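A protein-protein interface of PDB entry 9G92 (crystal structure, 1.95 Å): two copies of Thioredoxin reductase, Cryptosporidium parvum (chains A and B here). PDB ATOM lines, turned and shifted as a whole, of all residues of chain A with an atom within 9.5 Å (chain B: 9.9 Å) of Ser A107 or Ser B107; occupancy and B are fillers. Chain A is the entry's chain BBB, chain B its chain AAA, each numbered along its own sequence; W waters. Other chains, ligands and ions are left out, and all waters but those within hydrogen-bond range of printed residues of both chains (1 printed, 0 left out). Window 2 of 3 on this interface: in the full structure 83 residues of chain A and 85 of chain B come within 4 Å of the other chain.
Of chain B, only Thr B106 and Ser B107 come within 4 Å of Ser A107. Of the printed residues of chain A, Ser B107 touches Lys A105, Thr A106 and Ser A107. Of chain B, only Ile B95, Thr B106, Ser B107 and Ser B108 come within 4 Å of Thr A106. Printed residues of chain A within 4 Å of Ile B95: Thr A106. Of the printed residues of chain B, Phe A110 touches Gly B103 and His B104. Printed residues of chain B within 4 Å of Ile A95: Thr B106. Ala B99 touches none of the printed residues of chain A. His B96 touches none of the printed residues of chain A.
Among the printed residues, pairs that only touch across the chains: Ala A92 with His B104, Ile A95 with Thr B106, His A104 with Ser B108, His A104 with Ser B109, His A104 with Phe B110, Lys A105 with Ser B107, Lys A105 with Ser B108, Thr A106 with Ile B95, Thr A106 with Thr B106, Thr A106 with Ser B107, Ser A107 with Thr B106, Ser A108 with Lys B105, Ser A108 with Thr B106, Ser A109 with Gly B103, Ser A109 with His B104, Phe A110 with Gly B103 and Phe A110 with His B104.
N of His A104 is in hydrogen-bond range of O of Ala A99 (2.8 Å). OG1 of Thr A106 lies within hydrogen-bond range of O of His A104. N of His B104 sits at hydrogen-bond distance from O of Ala B99, at 2.8 Å.
His A104 touches Ser B108, but with the chains exchanged Ser A108 does not touch His B104 (4.8 Å). His A104 touches Ser B109, and with the chains exchanged Ser A109 touches His B104. Lys A105 touches Ser B108, and with the chains exchanged Ser A108 touches Lys B105. Thr A106 touches Ser B107, and with the chains exchanged Ser A107 touches Thr B106. 11 positions are printed for both chains. Of the 21 pairs that touch across the chains among the printed residues, 16 have their exchanged pair printed and touching as well.
Water W1 lies within hydrogen-bond range of the backbone NH of Lys A105 (3.0 Å) and the backbone carbonyl oxygen of Ser B109 (3.3 Å).
Hydrophobic or aromatic side chains of chain A within 4 Å of the printed part of chain B: Ala A92, Ile A95, His A104 and Phe A110. Along chain A the printed residues that touch a printed residue of chain B span positions 92 to 110. Of the 12 printed residues of chain B, 9 touch a printed residue of chain A. Hydrophobic or aromatic side chains of chain B that line the printed part of chain A: Ile B95, His B104 and Phe B110.
N of Ser A109 is in hydrogen-bond range of O of Lys B105, 3.0 Å away. The side-chain hydroxyl of Ser B108 sits at hydrogen-bond distance from the side-chain hydroxyl of Thr A106. The backbone carbonyl oxygen (O) of Ser B109 sits at hydrogen-bond distance from the backbone NH (N) of Lys A105 (3.3 Å). The side-chain hydroxyl (OG) of Ser B107 sits at hydrogen-bond distance from the side-chain hydroxyl (OG) of Ser A107, at 2.8 Å.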
ATOM      1  N   ALA A  92     -24.829 -26.983 -23.518  1.00  0.00           N
ATOM      2  CA  ALA A  92     -25.625 -25.902 -24.145  1.00  0.00           C
ATOM      3  C   ALA A  92     -26.646 -25.368 -23.136  1.00  0.00           C
ATOM      4  O   ALA A  92     -26.765 -24.125 -23.000  1.00  0.00           O
ATOM      5  CB  ALA A  92     -26.276 -26.388 -25.403  1.00  0.00           C
ATOM      6  N   ILE A  95     -24.896 -23.391 -20.322  1.00  0.00           N
ATOM      7  CA  ILE A  95     -24.432 -22.069 -20.831  1.00  0.00           C
ATOM      8  C   ILE A  95     -25.646 -21.134 -20.928  1.00  0.00           C
ATOM      9  O   ILE A  95     -25.538 -19.979 -20.470  1.00  0.00           O
ATOM     10  CB  ILE A  95     -23.690 -22.209 -22.179  1.00  0.00           C
ATOM     11  CG1 ILE A  95     -22.359 -22.931 -21.979  1.00  0.00           C
ATOM     12  CG2 ILE A  95     -23.520 -20.836 -22.830  1.00  0.00           C
ATOM     13  CD1 ILE A  95     -21.643 -23.328 -23.252  1.00  0.00           C
ATOM     14  N   HIS A  96     -26.761 -21.624 -21.463  1.00  0.00           N
ATOM     15  CA  HIS A  96     -27.995 -20.832 -21.685  1.00  0.00           C
ATOM     16  C   HIS A  96     -28.643 -20.472 -20.341  1.00  0.00           C
ATOM     17  O   HIS A  96     -28.959 -19.282 -20.130  1.00  0.00           O
ATOM     18  CB  HIS A  96     -28.968 -21.574 -22.612  1.00  0.00           C
ATOM     19  CG  HIS A  96     -30.220 -20.786 -22.839  1.00  0.00           C
ATOM     20  ND1 HIS A  96     -31.387 -21.020 -22.130  1.00  0.00           N
ATOM     21  CD2 HIS A  96     -30.466 -19.710 -23.622  1.00  0.00           C
ATOM     22  CE1 HIS A  96     -32.316 -20.153 -22.489  1.00  0.00           C
ATOM     23  NE2 HIS A  96     -31.776 -19.347 -23.417  1.00  0.00           N
ATOM     24  N   ALA A  99     -24.975 -20.466 -16.478  1.00  0.00           N
ATOM     25  CA  ALA A  99     -23.602 -19.931 -16.429  1.00  0.00           C
ATOM     26  C   ALA A  99     -23.618 -18.521 -15.813  1.00  0.00           C
ATOM     27  O   ALA A  99     -22.862 -18.276 -14.844  1.00  0.00           O
ATOM     28  CB  ALA A  99     -22.966 -19.948 -17.786  1.00  0.00           C
ATOM     29  N   GLN A 100     -24.466 -17.635 -16.316  1.00  0.00           N
ATOM     30  CA  GLN A 100     -24.519 -16.214 -15.854  1.00  0.00           C
ATOM     31  C   GLN A 100     -24.876 -16.154 -14.370  1.00  0.00           C
ATOM     32  O   GLN A 100     -24.245 -15.375 -13.653  1.00  0.00           O
ATOM     33  CB  GLN A 100     -25.519 -15.380 -16.673  1.00  0.00           C
ATOM     34  CG  GLN A 100     -25.637 -13.926 -16.171  1.00  0.00           C
ATOM     35  CD  GLN A 100     -26.240 -13.006 -17.214  1.00  0.00           C
ATOM     36  OE1 GLN A 100     -26.755 -13.434 -18.254  1.00  0.00           O
ATOM     37  NE2 GLN A 100     -26.139 -11.713 -16.973  1.00  0.00           N
ATOM     38  N   HIS A 104     -20.677 -16.612 -14.546  1.00  0.00           N
ATOM     39  CA  HIS A 104     -19.921 -16.825 -15.811  1.00  0.00           C
ATOM     40  C   HIS A 104     -20.763 -16.327 -16.990  1.00  0.00           C
ATOM     41  O   HIS A 104     -21.410 -17.193 -17.682  1.00  0.00           O
ATOM     42  CB  HIS A 104     -19.534 -18.293 -15.982  1.00  0.00           C
ATOM     43  CG  HIS A 104     -18.774 -18.833 -14.836  1.00  0.00           C
ATOM     44  ND1 HIS A 104     -17.406 -18.632 -14.713  1.00  0.00           N
ATOM     45  CD2 HIS A 104     -19.161 -19.612 -13.797  1.00  0.00           C
ATOM     46  CE1 HIS A 104     -16.998 -19.229 -13.596  1.00  0.00           C
ATOM     47  NE2 HIS A 104     -18.073 -19.812 -12.996  1.00  0.00           N
ATOM     48  N   LYS A 105     -20.685 -15.032 -17.306  1.00  0.00           N
ATOM     49  CA  LYS A 105     -21.428 -14.495 -18.467  1.00  0.00           C
ATOM     50  C   LYS A 105     -20.709 -15.018 -19.714  1.00  0.00           C
ATOM     51  O   LYS A 105     -19.480 -14.872 -19.846  1.00  0.00           O
ATOM     52  CB  LYS A 105     -21.597 -12.972 -18.445  1.00  0.00           C
ATOM     53  CG  LYS A 105     -22.637 -12.501 -19.460  1.00  0.00           C
ATOM     54  CD  LYS A 105     -22.615 -11.021 -19.730  1.00  0.00           C
ATOM     55  CE  LYS A 105     -23.412 -10.643 -20.965  1.00  0.00           C
ATOM     56  NZ  LYS A 105     -23.897  -9.241 -20.891  1.00  0.00           N
ATOM     57  N   THR A 106     -21.449 -15.758 -20.528  1.00  0.00           N
ATOM     58  CA  THR A 106     -20.870 -16.597 -21.587  1.00  0.00           C
ATOM     59  C   THR A 106     -21.694 -16.370 -22.845  1.00  0.00           C
ATOM     60  O   THR A 106     -22.902 -16.649 -22.801  1.00  0.00           O
ATOM     61  CB  THR A 106     -20.887 -18.083 -21.223  1.00  0.00           C
ATOM     62  OG1 THR A 106     -20.224 -18.215 -19.969  1.00  0.00           O
ATOM     63  CG2 THR A 106     -20.186 -18.943 -22.245  1.00  0.00           C
ATOM     64  N   SER A 107     -21.023 -15.968 -23.919  1.00  0.00           N
ATOM     65  CA  SER A 107     -21.564 -16.046 -25.295  1.00  0.00           C
ATOM     66  C   SER A 107     -20.972 -17.280 -25.990  1.00  0.00           C
ATOM     67  O   SER A 107     -19.786 -17.616 -25.796  1.00  0.00           O
ATOM     68  CB  SER A 107     -21.253 -14.792 -26.025  1.00  0.00           C
ATOM     69  OG  SER A 107     -19.857 -14.707 -26.126  1.00  0.00           O
ATOM     70  N   SER A 108     -21.782 -17.940 -26.792  1.00  0.00           N
ATOM     71  CA  SER A 108     -21.395 -19.224 -27.419  1.00  0.00           C
ATOM     72  C   SER A 108     -22.055 -19.335 -28.792  1.00  0.00           C
ATOM     73  O   SER A 108     -23.148 -18.776 -28.971  1.00  0.00           O
ATOM     74  CB  SER A 108     -21.765 -20.382 -26.521  1.00  0.00           C
ATOM     75  OG  SER A 108     -23.166 -20.559 -26.489  1.00  0.00           O
ATOM     76  N   SER A 109     -21.415 -20.055 -29.700  1.00  0.00           N
ATOM     77  CA  SER A 109     -22.067 -20.432 -30.966  1.00  0.00           C
ATOM     78  C   SER A 109     -21.700 -21.879 -31.252  1.00  0.00           C
ATOM     79  O   SER A 109     -20.566 -22.297 -30.971  1.00  0.00           O
ATOM     80  CB  SER A 109     -21.709 -19.523 -32.119  1.00  0.00           C
ATOM     81  OG  SER A 109     -20.310 -19.499 -32.271  1.00  0.00           O
ATOM     82  N   PHE A 110     -22.673 -22.607 -31.762  1.00  0.00           N
ATOM     83  CA  PHE A 110     -22.567 -24.069 -31.923  1.00  0.00           C
ATOM     84  C   PHE A 110     -22.179 -24.405 -33.365  1.00  0.00           C
ATOM     85  O   PHE A 110     -22.762 -23.836 -34.304  1.00  0.00           O
ATOM     86  CB  PHE A 110     -23.860 -24.711 -31.460  1.00  0.00           C
ATOM     87  CG  PHE A 110     -23.894 -26.180 -31.756  1.00  0.00           C
ATOM     88  CD1 PHE A 110     -23.026 -27.044 -31.102  1.00  0.00           C
ATOM     89  CD2 PHE A 110     -24.778 -26.696 -32.692  1.00  0.00           C
ATOM     90  CE1 PHE A 110     -23.048 -28.401 -31.362  1.00  0.00           C
ATOM     91  CE2 PHE A 110     -24.797 -28.061 -32.944  1.00  0.00           C
ATOM     92  CZ  PHE A 110     -23.930 -28.905 -32.288  1.00  0.00           C
ATOM     93  N   ILE B  95     -16.901 -25.162 -19.389  1.00  0.00           N
ATOM     94  CA  ILE B  95     -16.652 -24.099 -20.399  1.00  0.00           C
ATOM     95  C   ILE B  95     -15.195 -24.154 -20.861  1.00  0.00           C
ATOM     96  O   ILE B  95     -14.958 -24.133 -22.081  1.00  0.00           O
ATOM     97  CB  ILE B  95     -17.060 -22.713 -19.875  1.00  0.00           C
ATOM     98  CG1 ILE B  95     -18.571 -22.649 -19.674  1.00  0.00           C
ATOM     99  CG2 ILE B  95     -16.510 -21.615 -20.782  1.00  0.00           C
ATOM    100  CD1 ILE B  95     -19.017 -21.412 -18.896  1.00  0.00           C
ATOM    101  N   HIS B  96     -14.252 -24.234 -19.935  1.00  0.00           N
ATOM    102  CA  HIS B  96     -12.796 -24.208 -20.232  1.00  0.00           C
ATOM    103  C   HIS B  96     -12.380 -25.491 -20.965  1.00  0.00           C
ATOM    104  O   HIS B  96     -11.688 -25.378 -21.969  1.00  0.00           O
ATOM    105  CB  HIS B  96     -11.975 -23.974 -18.954  1.00  0.00           C
ATOM    106  CG  HIS B  96     -10.499 -24.024 -19.188  1.00  0.00           C
ATOM    107  ND1 HIS B  96      -9.743 -25.159 -18.935  1.00  0.00           N
ATOM    108  CD2 HIS B  96      -9.644 -23.114 -19.705  1.00  0.00           C
ATOM    109  CE1 HIS B  96      -8.478 -24.922 -19.247  1.00  0.00           C
ATOM    110  NE2 HIS B  96      -8.396 -23.680 -19.733  1.00  0.00           N
ATOM    111  N   ALA B  99     -16.525 -27.446 -23.621  1.00  0.00           N
ATOM    112  CA  ALA B  99     -17.521 -26.773 -24.473  1.00  0.00           C
ATOM    113  C   ALA B  99     -17.065 -26.810 -25.949  1.00  0.00           C
ATOM    114  O   ALA B  99     -17.863 -27.264 -26.775  1.00  0.00           O
ATOM    115  CB  ALA B  99     -17.771 -25.378 -23.994  1.00  0.00           C
ATOM    116  N   GLN B 100     -15.838 -26.405 -26.257  1.00  0.00           N
ATOM    117  CA  GLN B 100     -15.334 -26.348 -27.667  1.00  0.00           C
ATOM    118  C   GLN B 100     -15.324 -27.754 -28.290  1.00  0.00           C
ATOM    119  O   GLN B 100     -15.762 -27.896 -29.431  1.00  0.00           O
ATOM    120  CB  GLN B 100     -13.943 -25.714 -27.774  1.00  0.00           C
ATOM    121  CG  GLN B 100     -13.425 -25.664 -29.212  1.00  0.00           C
ATOM    122  CD  GLN B 100     -14.259 -24.716 -30.032  1.00  0.00           C
ATOM    123  OE1 GLN B 100     -13.894 -23.561 -30.203  1.00  0.00           O
ATOM    124  NE2 GLN B 100     -15.406 -25.172 -30.509  1.00  0.00           N
ATOM    125  N   GLY B 103     -18.558 -28.744 -29.498  1.00  0.00           N
ATOM    126  CA  GLY B 103     -18.975 -27.898 -30.629  1.00  0.00           C
ATOM    127  C   GLY B 103     -19.345 -26.486 -30.202  1.00  0.00           C
ATOM    128  O   GLY B 103     -19.713 -25.706 -31.093  1.00  0.00           O
ATOM    129  N   HIS B 104     -19.186 -26.128 -28.920  1.00  0.00           N
ATOM    130  CA  HIS B 104     -19.600 -24.798 -28.385  1.00  0.00           C
ATOM    131  C   HIS B 104     -18.371 -23.881 -28.247  1.00  0.00           C
ATOM    132  O   HIS B 104     -17.671 -23.922 -27.235  1.00  0.00           O
ATOM    133  CB  HIS B 104     -20.415 -24.969 -27.104  1.00  0.00           C
ATOM    134  CG  HIS B 104     -21.609 -25.843 -27.293  1.00  0.00           C
ATOM    135  ND1 HIS B 104     -22.799 -25.365 -27.818  1.00  0.00           N
ATOM    136  CD2 HIS B 104     -21.828 -27.133 -26.971  1.00  0.00           C
ATOM    137  CE1 HIS B 104     -23.690 -26.335 -27.839  1.00  0.00           C
ATOM    138  NE2 HIS B 104     -23.109 -27.441 -27.331  1.00  0.00           N
ATOM    139  N   LYS B 105     -18.152 -23.040 -29.251  1.00  0.00           N
ATOM    140  CA  LYS B 105     -17.090 -22.007 -29.211  1.00  0.00           C
ATOM    141  C   LYS B 105     -17.597 -20.930 -28.261  1.00  0.00           C
ATOM    142  O   LYS B 105     -18.649 -20.344 -28.574  1.00  0.00           O
ATOM    143  CB  LYS B 105     -16.829 -21.409 -30.604  1.00  0.00           C
ATOM    144  CG  LYS B 105     -15.832 -20.246 -30.614  1.00  0.00           C
ATOM    145  CD  LYS B 105     -14.433 -20.726 -30.265  1.00  0.00           C
ATOM    146  CE  LYS B 105     -13.495 -19.708 -29.647  1.00  0.00           C
ATOM    147  NZ  LYS B 105     -12.738 -18.954 -30.666  1.00  0.00           N
ATOM    148  N   THR B 106     -16.915 -20.688 -27.146  1.00  0.00           N
ATOM    149  CA  THR B 106     -17.455 -19.763 -26.104  1.00  0.00           C
ATOM    150  C   THR B 106     -16.479 -18.618 -25.801  1.00  0.00           C
ATOM    151  O   THR B 106     -15.279 -18.801 -25.921  1.00  0.00           O
ATOM    152  CB  THR B 106     -17.755 -20.490 -24.793  1.00  0.00           C
ATOM    153  OG1 THR B 106     -16.460 -20.855 -24.323  1.00  0.00           O
ATOM    154  CG2 THR B 106     -18.653 -21.690 -24.969  1.00  0.00           C
ATOM    155  N   SER B 107     -16.986 -17.474 -25.377  1.00  0.00           N
ATOM    156  CA  SER B 107     -16.139 -16.516 -24.629  1.00  0.00           C
ATOM    157  C   SER B 107     -16.819 -16.307 -23.287  1.00  0.00           C
ATOM    158  O   SER B 107     -18.050 -16.198 -23.240  1.00  0.00           O
ATOM    159  CB  SER B 107     -15.906 -15.232 -25.389  1.00  0.00           C
ATOM    160  OG  SER B 107     -17.121 -14.517 -25.467  1.00  0.00           O
ATOM    161  N   SER B 108     -16.038 -16.294 -22.219  1.00  0.00           N
ATOM    162  CA  SER B 108     -16.587 -16.280 -20.854  1.00  0.00           C
ATOM    163  C   SER B 108     -15.702 -15.436 -19.946  1.00  0.00           C
ATOM    164  O   SER B 108     -14.490 -15.390 -20.152  1.00  0.00           O
ATOM    165  CB  SER B 108     -16.704 -17.699 -20.361  1.00  0.00           C
ATOM    166  OG  SER B 108     -17.428 -17.734 -19.159  1.00  0.00           O
ATOM    167  N   SER B 109     -16.290 -14.810 -18.943  1.00  0.00           N
ATOM    168  CA  SER B 109     -15.508 -14.140 -17.877  1.00  0.00           C
ATOM    169  C   SER B 109     -16.289 -14.341 -16.589  1.00  0.00           C
ATOM    170  O   SER B 109     -17.522 -14.530 -16.665  1.00  0.00           O
ATOM    171  CB  SER B 109     -15.287 -12.661 -18.158  1.00  0.00           C
ATOM    172  OG  SER B 109     -16.538 -12.023 -18.306  1.00  0.00           O
ATOM    173  N   PHE B 110     -15.590 -14.320 -15.473  1.00  0.00           N
ATOM    174  CA  PHE B 110     -16.195 -14.601 -14.153  1.00  0.00           C
ATOM    175  C   PHE B 110     -16.318 -13.315 -13.341  1.00  0.00           C
ATOM    176  O   PHE B 110     -15.345 -12.520 -13.308  1.00  0.00           O
ATOM    177  CB  PHE B 110     -15.332 -15.631 -13.441  1.00  0.00           C
ATOM    178  CG  PHE B 110     -15.799 -15.905 -12.045  1.00  0.00           C
ATOM    179  CD1 PHE B 110     -17.048 -16.473 -11.823  1.00  0.00           C
ATOM    180  CD2 PHE B 110     -14.976 -15.608 -10.968  1.00  0.00           C
ATOM    181  CE1 PHE B 110     -17.463 -16.755 -10.533  1.00  0.00           C
ATOM    182  CE2 PHE B 110     -15.393 -15.897  -9.676  1.00  0.00           C
ATOM    183  CZ  PHE B 110     -16.634 -16.444  -9.456  1.00  0.00           C
HETATM  184  O   HOH W   1     -20.077 -12.785 -15.391  1.00  0.00           O
